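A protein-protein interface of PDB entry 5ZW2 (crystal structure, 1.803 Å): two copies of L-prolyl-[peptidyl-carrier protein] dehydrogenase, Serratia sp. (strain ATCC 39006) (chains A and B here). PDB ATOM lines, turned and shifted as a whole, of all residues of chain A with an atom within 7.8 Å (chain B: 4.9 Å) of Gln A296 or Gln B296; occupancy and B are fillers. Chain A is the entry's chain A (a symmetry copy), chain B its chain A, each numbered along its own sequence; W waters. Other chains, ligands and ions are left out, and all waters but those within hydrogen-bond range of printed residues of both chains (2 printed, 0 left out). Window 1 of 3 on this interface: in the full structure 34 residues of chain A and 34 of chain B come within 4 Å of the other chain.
OH of Tyr B328 sits at hydrogen-bond distance from OE1 of Gln A296, at 2.7 Å. The side-chain amide oxygen of Gln B296 sits close to the side-chain amide oxygen of Gln A296, 3.3 Å away. The side-chain carboxylate of Glu B295 is in salt-bridge range of the guanidinium group of Arg A303 (2.8 Å). OE1 of Gln B296 sits at hydrogen-bond distance from OH of Tyr A328 (2.7 Å).
NZ of Lys A291 lies within salt-bridge range of OE2 of Glu A295, at 2.8 Å. The backbone carbonyl oxygen of Met A300 lies within hydrogen-bond range of the side-chain hydroxyl of Ser A321 (3.0 Å). O of Leu A292 is in hydrogen-bond range of NE2 of Gln A296, at 3.0 Å. NH1 of Arg B298 lies within salt-bridge range of OE2 of Glu B295 (3.3 Å). O of Leu B292 lies within hydrogen-bond range of NE2 of Gln B296 (3.0 Å). The side-chain carboxylate (OE2) of Glu A295 is in salt-bridge range of the guanidinium group (NH1) of Arg A298 (3.3 Å).
Met B300 touches Glu A295. Gln A296 touches Met B300. Gln A296 touches Leu B324. Leu A299 touches Met B300 (CD1 to SD, 3.8 Å). Glu B295 touches Met A300. Met A300 touches Gln B296. Met A300 touches Leu B299 (SD to CD1, 3.8 Å). Arg A303 touches Leu B299. Leu B292 touches Met A320 (CD2 to CB, 3.6 Å). Leu A324 touches Gln B296.
Gln A296 touches just these residues of chain B: Gln B296, Met B300, Leu B324 and Tyr B328. Of the printed residues of chain B, Met A300 touches Glu B295 (3.7 Å), Gln B296 (3.8 Å) and Leu B299 (3.8 Å). Of the printed residues of chain B, Met A320 touches Leu B292. Of the printed residues of chain A, Leu B292 touches Met A320. Printed residues of chain B within 4 Å of Arg A303: Glu B295 and Leu B299. Printed residues of chain A within 4 Å of Tyr B328: Gln A296. Arg B293 touches none of the printed residues of chain A. Cys A297 touches none of the printed residues of chain B. The nearest residue of chain A that does not touch Gln B296 is Cys A297 (4.7 Å). The nearest printed residue of chain A that does not touch Leu B324 is Leu A292 (4.04 Å).
Hydrophobic or aromatic side chains of chain B within 4 Å of the printed part of chain A: Leu B292, Leu B299, Met B300, Leu B324 and Tyr B328. Of the 22 printed residues of chain A, 8 touch a printed residue of chain B. Printed residues of chain A that touch a printed residue of chain B: Glu A295, Gln A296, Leu A299, Met A300, Arg A303, Met A320, Leu A324 and Tyr A328. Among the printed residues, 14 pairs touch across the chains.
Glu A295 touches Met B300, and with the chains exchanged Met A300 touches Glu B295. Gln B296 touches its own counterpart, Gln A296. Gln A296 touches Met B300, and with the chains exchanged Met A300 touches Gln B296. Gln A296 touches Leu B324, and with the chains exchanged Leu A324 touches Gln B296. Positions printed for both chains: 292, 293, 294, 295, 296, 297, 298, 299, 300, 324 and 328.
Water W2 lies within hydrogen-bond range of OE1 of Glu B295 (2.6 Å), NH1 of Arg A303 (3.1 Å) and NH1 of Arg B298 (3.1 Å). Water W1 lies within hydrogen-bond range of OH of Tyr B328 and OH of Tyr A328.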
ATOM      1  N   LEU A 256     -31.453 -16.422 -24.296  1.00  0.00           N
ATOM      2  CA  LEU A 256     -30.177 -15.910 -24.828  1.00  0.00           C
ATOM      3  C   LEU A 256     -29.436 -17.000 -25.602  1.00  0.00           C
ATOM      4  O   LEU A 256     -28.803 -16.744 -26.623  1.00  0.00           O
ATOM      5  CB  LEU A 256     -29.324 -15.376 -23.650  1.00  0.00           C
ATOM      6  CG  LEU A 256     -27.927 -14.844 -24.020  1.00  0.00           C
ATOM      7  CD1 LEU A 256     -28.018 -13.764 -25.117  1.00  0.00           C
ATOM      8  CD2 LEU A 256     -27.219 -14.274 -22.776  1.00  0.00           C
ATOM      9  N   ILE A 288     -19.291 -12.051 -29.894  1.00  0.00           N
ATOM     10  CA  ILE A 288     -18.471 -12.627 -28.839  1.00  0.00           C
ATOM     11  C   ILE A 288     -18.927 -12.117 -27.478  1.00  0.00           C
ATOM     12  O   ILE A 288     -18.920 -12.869 -26.506  1.00  0.00           O
ATOM     13  CB  ILE A 288     -16.975 -12.353 -29.124  1.00  0.00           C
ATOM     14  CG1 ILE A 288     -16.515 -13.276 -30.266  1.00  0.00           C
ATOM     15  CG2 ILE A 288     -16.133 -12.651 -27.836  1.00  0.00           C
ATOM     16  CD1 ILE A 288     -15.315 -12.736 -30.976  1.00  0.00           C
ATOM     17  N   ASP A 289     -19.274 -10.819 -27.361  1.00  0.00           N
ATOM     18  CA  ASP A 289     -19.853 -10.334 -26.102  1.00  0.00           C
ATOM     19  C   ASP A 289     -21.090 -11.126 -25.715  1.00  0.00           C
ATOM     20  O   ASP A 289     -21.297 -11.440 -24.537  1.00  0.00           O
ATOM     21  CB  ASP A 289     -20.202  -8.835 -26.209  1.00  0.00           C
ATOM     22  CG  ASP A 289     -18.996  -7.950 -26.084  1.00  0.00           C
ATOM     23  OD1 ASP A 289     -19.080  -6.800 -26.574  1.00  0.00           O
ATOM     24  OD2 ASP A 289     -17.953  -8.444 -25.591  1.00  0.00           O
ATOM     25  N   MET A 290     -21.970 -11.410 -26.687  1.00  0.00           N
ATOM     26  CA  MET A 290     -23.166 -12.179 -26.349  1.00  0.00           C
ATOM     27  C   MET A 290     -22.789 -13.547 -25.797  1.00  0.00           C
ATOM     28  O   MET A 290     -23.372 -14.009 -24.822  1.00  0.00           O
ATOM     29  CB  MET A 290     -24.036 -12.408 -27.618  1.00  0.00           C
ATOM     30  CG  MET A 290     -24.514 -11.070 -28.181  1.00  0.00           C
ATOM     31  SD  MET A 290     -25.263 -11.252 -29.842  1.00  0.00           S
ATOM     32  CE  MET A 290     -26.766 -12.128 -29.429  1.00  0.00           C
ATOM     33  N   LYS A 291     -21.815 -14.215 -26.436  1.00  0.00           N
ATOM     34  CA  LYS A 291     -21.364 -15.521 -25.952  1.00  0.00           C
ATOM     35  C   LYS A 291     -20.703 -15.411 -24.571  1.00  0.00           C
ATOM     36  O   LYS A 291     -20.945 -16.251 -23.690  1.00  0.00           O
ATOM     37  CB  LYS A 291     -20.392 -16.118 -27.016  1.00  0.00           C
ATOM     38  CG  LYS A 291     -19.606 -17.466 -26.624  1.00  0.00           C
ATOM     39  CD  LYS A 291     -20.548 -18.626 -26.493  1.00  0.00           C
ATOM     40  CE  LYS A 291     -19.793 -20.076 -26.394  1.00  0.00           C
ATOM     41  NZ  LYS A 291     -20.992 -20.985 -26.097  1.00  0.00           N
ATOM     42  N   LEU A 292     -19.834 -14.420 -24.375  1.00  0.00           N
ATOM     43  CA  LEU A 292     -19.234 -14.231 -23.024  1.00  0.00           C
ATOM     44  C   LEU A 292     -20.320 -14.063 -21.961  1.00  0.00           C
ATOM     45  O   LEU A 292     -20.250 -14.654 -20.875  1.00  0.00           O
ATOM     46  CB  LEU A 292     -18.331 -13.003 -23.023  1.00  0.00           C
ATOM     47  CG  LEU A 292     -17.033 -13.096 -23.832  1.00  0.00           C
ATOM     48  CD1 LEU A 292     -16.379 -11.726 -23.985  1.00  0.00           C
ATOM     49  CD2 LEU A 292     -16.034 -14.106 -23.155  1.00  0.00           C
ATOM     50  N   ARG A 293     -21.316 -13.229 -22.241  1.00  0.00           N
ATOM     51  CA  ARG A 293     -22.412 -13.033 -21.279  1.00  0.00           C
ATOM     52  C   ARG A 293     -23.126 -14.333 -20.975  1.00  0.00           C
ATOM     53  O   ARG A 293     -23.500 -14.605 -19.820  1.00  0.00           O
ATOM     54  CB  ARG A 293     -23.431 -12.020 -21.851  1.00  0.00           C
ATOM     55  CG  ARG A 293     -22.835 -10.566 -21.966  1.00  0.00           C
ATOM     56  CD  ARG A 293     -23.909  -9.733 -22.746  1.00  0.00           C
ATOM     57  NE  ARG A 293     -23.320  -8.438 -23.096  1.00  0.00           N
ATOM     58  CZ  ARG A 293     -23.475  -7.824 -24.270  1.00  0.00           C
ATOM     59  NH1 ARG A 293     -24.228  -8.371 -25.214  1.00  0.00           N
ATOM     60  NH2 ARG A 293     -22.808  -6.674 -24.513  1.00  0.00           N
ATOM     61  N   LEU A 294     -23.462 -15.085 -22.024  1.00  0.00           N
ATOM     62  CA  LEU A 294     -24.247 -16.293 -21.803  1.00  0.00           C
ATOM     63  C   LEU A 294     -23.475 -17.257 -20.893  1.00  0.00           C
ATOM     64  O   LEU A 294     -24.036 -17.828 -19.950  1.00  0.00           O
ATOM     65  CB  LEU A 294     -24.557 -16.948 -23.174  1.00  0.00           C
ATOM     66  CG  LEU A 294     -25.205 -18.339 -23.069  1.00  0.00           C
ATOM     67  CD1 LEU A 294     -26.575 -18.204 -22.444  1.00  0.00           C
ATOM     68  CD2 LEU A 294     -25.357 -18.947 -24.493  1.00  0.00           C
ATOM     69  N   GLU A 295     -22.187 -17.465 -21.178  1.00  0.00           N
ATOM     70  CA  GLU A 295     -21.457 -18.462 -20.394  1.00  0.00           C
ATOM     71  C   GLU A 295     -21.323 -17.993 -18.953  1.00  0.00           C
ATOM     72  O   GLU A 295     -21.424 -18.805 -18.018  1.00  0.00           O
ATOM     73  CB  GLU A 295     -20.080 -18.753 -21.024  1.00  0.00           C
ATOM     74  CG  GLU A 295     -20.128 -19.348 -22.460  1.00  0.00           C
ATOM     75  CD  GLU A 295     -21.088 -20.560 -22.555  1.00  0.00           C
ATOM     76  OE1 GLU A 295     -21.039 -21.433 -21.669  1.00  0.00           O
ATOM     77  OE2 GLU A 295     -21.908 -20.647 -23.515  1.00  0.00           O
ATOM     78  N   GLN A 296     -21.036 -16.703 -18.757  1.00  0.00           N
ATOM     79  CA  GLN A 296     -20.838 -16.198 -17.391  1.00  0.00           C
ATOM     80  C   GLN A 296     -22.124 -16.262 -16.579  1.00  0.00           C
ATOM     81  O   GLN A 296     -22.112 -16.684 -15.416  1.00  0.00           O
ATOM     82  CB  GLN A 296     -20.363 -14.745 -17.436  1.00  0.00           C
ATOM     83  CG  GLN A 296     -18.886 -14.654 -17.905  1.00  0.00           C
ATOM     84  CD  GLN A 296     -18.537 -13.145 -18.022  1.00  0.00           C
ATOM     85  OE1 GLN A 296     -17.908 -12.546 -17.134  1.00  0.00           O
ATOM     86  NE2 GLN A 296     -18.998 -12.532 -19.098  1.00  0.00           N
ATOM     87  N   CYS A 297     -23.245 -15.784 -17.150  1.00  0.00           N
ATOM     88  CA  CYS A 297     -24.427 -15.730 -16.299  1.00  0.00           C
ATOM     89  C   CYS A 297     -25.007 -17.118 -16.106  1.00  0.00           C
ATOM     90  O   CYS A 297     -25.591 -17.387 -15.056  1.00  0.00           O
ATOM     91  CB  CYS A 297     -25.494 -14.733 -16.809  1.00  0.00           C
ATOM     92  SG  CYS A 297     -26.360 -15.208 -18.375  1.00  0.00           S
ATOM     93  N   ARG A 298     -24.804 -18.014 -17.061  1.00  0.00           N
ATOM     94  CA  ARG A 298     -25.294 -19.372 -16.842  1.00  0.00           C
ATOM     95  C   ARG A 298     -24.550 -20.003 -15.672  1.00  0.00           C
ATOM     96  O   ARG A 298     -25.156 -20.661 -14.822  1.00  0.00           O
ATOM     97  CB  ARG A 298     -25.081 -20.245 -18.101  1.00  0.00           C
ATOM     98  CG  ARG A 298     -25.601 -21.651 -17.895  1.00  0.00           C
ATOM     99  CD  ARG A 298     -26.187 -22.328 -19.174  1.00  0.00           C
ATOM    100  NE  ARG A 298     -25.279 -22.210 -20.272  1.00  0.00           N
ATOM    101  CZ  ARG A 298     -25.605 -22.182 -21.551  1.00  0.00           C
ATOM    102  NH1 ARG A 298     -24.614 -22.046 -22.382  1.00  0.00           N
ATOM    103  NH2 ARG A 298     -26.856 -22.268 -22.004  1.00  0.00           N
ATOM    104  N   LEU A 299     -23.213 -19.821 -15.627  1.00  0.00           N
ATOM    105  CA  LEU A 299     -22.469 -20.411 -14.507  1.00  0.00           C
ATOM    106  C   LEU A 299     -22.871 -19.794 -13.177  1.00  0.00           C
ATOM    107  O   LEU A 299     -22.945 -20.509 -12.148  1.00  0.00           O
ATOM    108  CB  LEU A 299     -20.953 -20.264 -14.722  1.00  0.00           C
ATOM    109  CG  LEU A 299     -20.445 -21.166 -15.848  1.00  0.00           C
ATOM    110  CD1 LEU A 299     -19.036 -20.757 -16.134  1.00  0.00           C
ATOM    111  CD2 LEU A 299     -20.462 -22.612 -15.382  1.00  0.00           C
ATOM    112  N   MET A 300     -23.065 -18.478 -13.143  1.00  0.00           N
ATOM    113  CA  MET A 300     -23.495 -17.844 -11.889  1.00  0.00           C
ATOM    114  C   MET A 300     -24.857 -18.371 -11.454  1.00  0.00           C
ATOM    115  O   MET A 300     -25.118 -18.555 -10.246  1.00  0.00           O
ATOM    116  CB  MET A 300     -23.531 -16.311 -12.076  1.00  0.00           C
ATOM    117  CG  MET A 300     -22.149 -15.706 -12.317  1.00  0.00           C
ATOM    118  SD  MET A 300     -21.180 -15.688 -10.763  1.00  0.00           S
ATOM    119  CE  MET A 300     -22.033 -14.335  -9.857  1.00  0.00           C
ATOM    120  N   LEU A 301     -25.754 -18.571 -12.418  1.00  0.00           N
ATOM    121  CA  LEU A 301     -27.093 -19.090 -12.063  1.00  0.00           C
ATOM    122  C   LEU A 301     -26.977 -20.499 -11.495  1.00  0.00           C
ATOM    123  O   LEU A 301     -27.575 -20.829 -10.456  1.00  0.00           O
ATOM    124  CB  LEU A 301     -27.996 -19.107 -13.303  1.00  0.00           C
ATOM    125  CG  LEU A 301     -29.337 -19.843 -13.100  1.00  0.00           C
ATOM    126  CD1 LEU A 301     -30.190 -19.110 -12.084  1.00  0.00           C
ATOM    127  CD2 LEU A 301     -30.070 -20.018 -14.364  1.00  0.00           C
ATOM    128  N   TYR A 302     -26.233 -21.348 -12.189  1.00  0.00           N
ATOM    129  CA  TYR A 302     -26.108 -22.731 -11.741  1.00  0.00           C
ATOM    130  C   TYR A 302     -25.494 -22.783 -10.366  1.00  0.00           C
ATOM    131  O   TYR A 302     -25.889 -23.609  -9.543  1.00  0.00           O
ATOM    132  CB  TYR A 302     -25.230 -23.550 -12.674  1.00  0.00           C
ATOM    133  CG  TYR A 302     -25.845 -23.851 -14.042  1.00  0.00           C
ATOM    134  CD1 TYR A 302     -27.159 -23.497 -14.323  1.00  0.00           C
ATOM    135  CD2 TYR A 302     -25.073 -24.405 -15.036  1.00  0.00           C
ATOM    136  CE1 TYR A 302     -27.716 -23.715 -15.622  1.00  0.00           C
ATOM    137  CE2 TYR A 302     -25.616 -24.674 -16.317  1.00  0.00           C
ATOM    138  CZ  TYR A 302     -26.947 -24.339 -16.574  1.00  0.00           C
ATOM    139  OH  TYR A 302     -27.465 -24.586 -17.828  1.00  0.00           O
ATOM    140  N   ARG A 303     -24.507 -21.934 -10.106  1.00  0.00           N
ATOM    141  CA  ARG A 303     -23.889 -21.991  -8.778  1.00  0.00           C
ATOM    142  C   ARG A 303     -24.847 -21.505  -7.702  1.00  0.00           C
ATOM    143  O   ARG A 303     -24.885 -22.071  -6.595  1.00  0.00           O
ATOM    144  CB  ARG A 303     -22.571 -21.198  -8.736  1.00  0.00           C
ATOM    145  CG  ARG A 303     -21.993 -21.234  -7.301  1.00  0.00           C
ATOM    146  CD  ARG A 303     -20.533 -20.790  -7.326  1.00  0.00           C
ATOM    147  NE  ARG A 303     -20.539 -19.352  -7.298  1.00  0.00           N
ATOM    148  CZ  ARG A 303     -19.463 -18.568  -7.201  1.00  0.00           C
ATOM    149  NH1 ARG A 303     -18.237 -19.081  -7.129  1.00  0.00           N
ATOM    150  NH2 ARG A 303     -19.626 -17.256  -7.174  1.00  0.00           N
ATOM    151  N   MET A 320     -27.001 -11.648  -7.487  1.00  0.00           N
ATOM    152  CA  MET A 320     -26.040 -11.431  -8.579  1.00  0.00           C
ATOM    153  C   MET A 320     -26.513 -12.070  -9.895  1.00  0.00           C
ATOM    154  O   MET A 320     -26.350 -11.499 -10.986  1.00  0.00           O
ATOM    155  CB  MET A 320     -24.663 -11.986  -8.205  1.00  0.00           C
ATOM    156  CG  MET A 320     -24.050 -11.204  -7.041  1.00  0.00           C
ATOM    157  SD  MET A 320     -22.305 -11.793  -6.746  1.00  0.00           S
ATOM    158  CE  MET A 320     -22.507 -13.327  -5.994  1.00  0.00           C
ATOM    159  N   SER A 321     -27.041 -13.294  -9.810  1.00  0.00           N
ATOM    160  CA  SER A 321     -27.510 -13.975 -11.017  1.00  0.00           C
ATOM    161  C   SER A 321     -28.644 -13.219 -11.680  1.00  0.00           C
ATOM    162  O   SER A 321     -28.671 -13.078 -12.913  1.00  0.00           O
ATOM    163  CB  SER A 321     -27.972 -15.384 -10.662  1.00  0.00           C
ATOM    164  OG  SER A 321     -26.832 -16.141 -10.413  1.00  0.00           O
ATOM    165  N   LEU A 324     -27.178 -10.117 -13.434  1.00  0.00           N
ATOM    166  CA  LEU A 324     -26.389 -10.390 -14.639  1.00  0.00           C
ATOM    167  C   LEU A 324     -27.278 -10.894 -15.766  1.00  0.00           C
ATOM    168  O   LEU A 324     -27.156 -10.460 -16.928  1.00  0.00           O
ATOM    169  CB  LEU A 324     -25.319 -11.431 -14.366  1.00  0.00           C
ATOM    170  CG  LEU A 324     -24.242 -10.915 -13.381  1.00  0.00           C
ATOM    171  CD1 LEU A 324     -23.358 -12.124 -13.017  1.00  0.00           C
ATOM    172  CD2 LEU A 324     -23.359  -9.845 -14.106  1.00  0.00           C
ATOM    173  N   ILE A 325     -28.148 -11.853 -15.448  1.00  0.00           N
ATOM    174  CA  ILE A 325     -28.956 -12.447 -16.521  1.00  0.00           C
ATOM    175  C   ILE A 325     -29.768 -11.362 -17.210  1.00  0.00           C
ATOM    176  O   ILE A 325     -29.869 -11.305 -18.439  1.00  0.00           O
ATOM    177  CB  ILE A 325     -29.876 -13.516 -15.919  1.00  0.00           C
ATOM    178  CG1 ILE A 325     -29.051 -14.781 -15.600  1.00  0.00           C
ATOM    179  CG2 ILE A 325     -30.979 -13.911 -16.939  1.00  0.00           C
ATOM    180  CD1 ILE A 325     -29.937 -15.743 -14.655  1.00  0.00           C
ATOM    181  N   TYR A 328     -27.654  -8.788 -19.130  1.00  0.00           N
ATOM    182  CA  TYR A 328     -27.078  -9.419 -20.327  1.00  0.00           C
ATOM    183  C   TYR A 328     -28.154  -9.724 -21.357  1.00  0.00           C
ATOM    184  O   TYR A 328     -27.903  -9.654 -22.568  1.00  0.00           O
ATOM    185  CB  TYR A 328     -26.340 -10.712 -19.973  1.00  0.00           C
ATOM    186  CG  TYR A 328     -25.034 -10.492 -19.208  1.00  0.00           C
ATOM    187  CD1 TYR A 328     -24.474  -9.234 -19.108  1.00  0.00           C
ATOM    188  CD2 TYR A 328     -24.412 -11.573 -18.587  1.00  0.00           C
ATOM    189  CE1 TYR A 328     -23.244  -9.038 -18.365  1.00  0.00           C
ATOM    190  CE2 TYR A 328     -23.180 -11.409 -17.849  1.00  0.00           C
ATOM    191  CZ  TYR A 328     -22.604 -10.148 -17.783  1.00  0.00           C
ATOM    192  OH  TYR A 328     -21.407  -9.966 -17.100  1.00  0.00           O
ATOM    193  N   LEU B 292     -18.895  -8.803  -8.848  1.00  0.00           N
ATOM    194  CA  LEU B 292     -19.482  -9.544  -9.999  1.00  0.00           C
ATOM    195  C   LEU B 292     -18.388 -10.047 -10.942  1.00  0.00           C
ATOM    196  O   LEU B 292     -18.416 -11.197 -11.401  1.00  0.00           O
ATOM    197  CB  LEU B 292     -20.437  -8.639 -10.769  1.00  0.00           C
ATOM    198  CG  LEU B 292     -21.741  -8.249 -10.067  1.00  0.00           C
ATOM    199  CD1 LEU B 292     -22.455  -7.125 -10.813  1.00  0.00           C
ATOM    200  CD2 LEU B 292     -22.686  -9.500  -9.930  1.00  0.00           C
ATOM    201  N   ARG B 293     -17.433  -9.185 -11.273  1.00  0.00           N
ATOM    202  CA  ARG B 293     -16.332  -9.601 -12.156  1.00  0.00           C
ATOM    203  C   ARG B 293     -15.558 -10.765 -11.572  1.00  0.00           C
ATOM    204  O   ARG B 293     -15.156 -11.694 -12.294  1.00  0.00           O
ATOM    205  CB  ARG B 293     -15.365  -8.414 -12.377  1.00  0.00           C
ATOM    206  CG  ARG B 293     -16.023  -7.247 -13.206  1.00  0.00           C
ATOM    207  CD  ARG B 293     -14.998  -6.063 -13.153  1.00  0.00           C
ATOM    208  NE  ARG B 293     -15.646  -4.869 -13.700  1.00  0.00           N
ATOM    209  CZ  ARG B 293     -15.535  -3.642 -13.189  1.00  0.00           C
ATOM    210  NH1 ARG B 293     -14.774  -3.429 -12.125  1.00  0.00           N
ATOM    211  NH2 ARG B 293     -16.254  -2.630 -13.724  1.00  0.00           N
ATOM    212  N   LEU B 294     -15.207 -10.660 -10.290  1.00  0.00           N
ATOM    213  CA  LEU B 294     -14.368 -11.698  -9.702  1.00  0.00           C
ATOM    214  C   LEU B 294     -15.085 -13.052  -9.776  1.00  0.00           C
ATOM    215  O   LEU B 294     -14.486 -14.068 -10.148  1.00  0.00           O
ATOM    216  CB  LEU B 294     -14.052 -11.314  -8.233  1.00  0.00           C
ATOM    217  CG  LEU B 294     -13.344 -12.423  -7.437  1.00  0.00           C
ATOM    218  CD1 LEU B 294     -11.972 -12.660  -8.026  1.00  0.00           C
ATOM    219  CD2 LEU B 294     -13.188 -11.977  -5.955  1.00  0.00           C
ATOM    220  N   GLU B 295     -16.367 -13.085  -9.405  1.00  0.00           N
ATOM    221  CA  GLU B 295     -17.042 -14.382  -9.362  1.00  0.00           C
ATOM    222  C   GLU B 295     -17.174 -14.945 -10.769  1.00  0.00           C
ATOM    223  O   GLU B 295     -17.025 -16.162 -10.973  1.00  0.00           O
ATOM    224  CB  GLU B 295     -18.416 -14.263  -8.671  1.00  0.00           C
ATOM    225  CG  GLU B 295     -18.364 -13.803  -7.186  1.00  0.00           C
ATOM    226  CD  GLU B 295     -17.355 -14.634  -6.355  1.00  0.00           C
ATOM    227  OE1 GLU B 295     -17.353 -15.872  -6.480  1.00  0.00           O
ATOM    228  OE2 GLU B 295     -16.547 -14.054  -5.572  1.00  0.00           O
ATOM    229  N   GLN B 296     -17.513 -14.090 -11.738  1.00  0.00           N
ATOM    230  CA  GLN B 296     -17.711 -14.581 -13.109  1.00  0.00           C
ATOM    231  C   GLN B 296     -16.412 -15.093 -13.713  1.00  0.00           C
ATOM    232  O   GLN B 296     -16.388 -16.159 -14.341  1.00  0.00           O
ATOM    233  CB  GLN B 296     -18.248 -13.455 -13.994  1.00  0.00           C
ATOM    234  CG  GLN B 296     -19.734 -13.148 -13.668  1.00  0.00           C
ATOM    235  CD  GLN B 296     -20.148 -11.927 -14.534  1.00  0.00           C
ATOM    236  OE1 GLN B 296     -20.788 -12.059 -15.591  1.00  0.00           O
ATOM    237  NE2 GLN B 296     -19.730 -10.750 -14.103  1.00  0.00           N
ATOM    238  N   CYS B 297     -15.320 -14.314 -13.596  1.00  0.00           N
ATOM    239  CA  CYS B 297     -14.129 -14.765 -14.304  1.00  0.00           C
ATOM    240  C   CYS B 297     -13.488 -15.932 -13.576  1.00  0.00           C
ATOM    241  O   CYS B 297     -12.877 -16.783 -14.223  1.00  0.00           O
ATOM    242  CB  CYS B 297     -13.113 -13.627 -14.563  1.00  0.00           C
ATOM    243  SG  CYS B 297     -12.252 -12.958 -13.066  1.00  0.00           S
ATOM    244  N   ARG B 298     -13.667 -16.021 -12.267  1.00  0.00           N
ATOM    245  CA  ARG B 298     -13.117 -17.184 -11.577  1.00  0.00           C
ATOM    246  C   ARG B 298     -13.815 -18.447 -12.064  1.00  0.00           C
ATOM    247  O   ARG B 298     -13.169 -19.469 -12.310  1.00  0.00           O
ATOM    248  CB  ARG B 298     -13.312 -17.062 -10.047  1.00  0.00           C
ATOM    249  CG  ARG B 298     -12.730 -18.253  -9.318  1.00  0.00           C
ATOM    250  CD  ARG B 298     -12.135 -17.934  -7.910  1.00  0.00           C
ATOM    251  NE  ARG B 298     -13.064 -17.181  -7.126  1.00  0.00           N
ATOM    252  CZ  ARG B 298     -12.759 -16.331  -6.163  1.00  0.00           C
ATOM    253  NH1 ARG B 298     -13.767 -15.738  -5.594  1.00  0.00           N
ATOM    254  NH2 ARG B 298     -11.513 -16.056  -5.778  1.00  0.00           N
ATOM    255  N   LEU B 299     -15.158 -18.392 -12.195  1.00  0.00           N
ATOM    256  CA  LEU B 299     -15.859 -19.591 -12.670  1.00  0.00           C
ATOM    257  C   LEU B 299     -15.463 -19.947 -14.094  1.00  0.00           C
ATOM    258  O   LEU B 299     -15.344 -21.151 -14.433  1.00  0.00           O
ATOM    259  CB  LEU B 299     -17.383 -19.405 -12.575  1.00  0.00           C
ATOM    260  CG  LEU B 299     -17.870 -19.403 -11.126  1.00  0.00           C
ATOM    261  CD1 LEU B 299     -19.299 -18.965 -11.144  1.00  0.00           C
ATOM    262  CD2 LEU B 299     -17.785 -20.812 -10.562  1.00  0.00           C
ATOM    263  N   MET B 300     -15.325 -18.949 -14.962  1.00  0.00           N
ATOM    264  CA  MET B 300     -14.903 -19.242 -16.339  1.00  0.00           C
ATOM    265  C   MET B 300     -13.514 -19.867 -16.359  1.00  0.00           C
ATOM    266  O   MET B 300     -13.226 -20.768 -17.176  1.00  0.00           O
ATOM    267  CB  MET B 300     -14.934 -17.942 -17.172  1.00  0.00           C
ATOM    268  CG  MET B 300     -16.345 -17.381 -17.352  1.00  0.00           C
ATOM    269  SD  MET B 300     -17.290 -18.400 -18.545  1.00  0.00           S
ATOM    270  CE  MET B 300     -16.481 -17.900 -20.119  1.00  0.00           C
ATOM    271  N   LEU B 324     -11.574 -12.157 -20.131  1.00  0.00           N
ATOM    272  CA  LEU B 324     -12.369 -11.632 -19.016  1.00  0.00           C
ATOM    273  C   LEU B 324     -11.477 -11.264 -17.840  1.00  0.00           C
ATOM    274  O   LEU B 324     -11.635 -10.195 -17.220  1.00  0.00           O
ATOM    275  CB  LEU B 324     -13.390 -12.652 -18.547  1.00  0.00           C
ATOM    276  CG  LEU B 324     -14.473 -12.929 -19.618  1.00  0.00           C
ATOM    277  CD1 LEU B 324     -15.299 -14.129 -19.114  1.00  0.00           C
ATOM    278  CD2 LEU B 324     -15.411 -11.681 -19.728  1.00  0.00           C
ATOM    279  N   TYR B 328     -11.242  -7.484 -16.597  1.00  0.00           N
ATOM    280  CA  TYR B 328     -11.808  -7.231 -15.264  1.00  0.00           C
ATOM    281  C   TYR B 328     -10.736  -6.763 -14.293  1.00  0.00           C
ATOM    282  O   TYR B 328     -11.009  -5.948 -13.401  1.00  0.00           O
ATOM    283  CB  TYR B 328     -12.486  -8.482 -14.702  1.00  0.00           C
ATOM    284  CG  TYR B 328     -13.788  -8.855 -15.411  1.00  0.00           C
ATOM    285  CD1 TYR B 328     -14.399  -7.975 -16.282  1.00  0.00           C
ATOM    286  CD2 TYR B 328     -14.355 -10.109 -15.191  1.00  0.00           C
ATOM    287  CE1 TYR B 328     -15.625  -8.349 -16.960  1.00  0.00           C
ATOM    288  CE2 TYR B 328     -15.581 -10.506 -15.845  1.00  0.00           C
ATOM    289  CZ  TYR B 328     -16.208  -9.602 -16.691  1.00  0.00           C
ATOM    290  OH  TYR B 328     -17.402  -9.948 -17.315  1.00  0.00           O
HETATM  291  O   HOH W   1     -19.446  -8.221 -17.833  1.00  0.00           O
HETATM  292  O   HOH W   2     -16.118 -17.792  -5.224  1.00  0.00           O
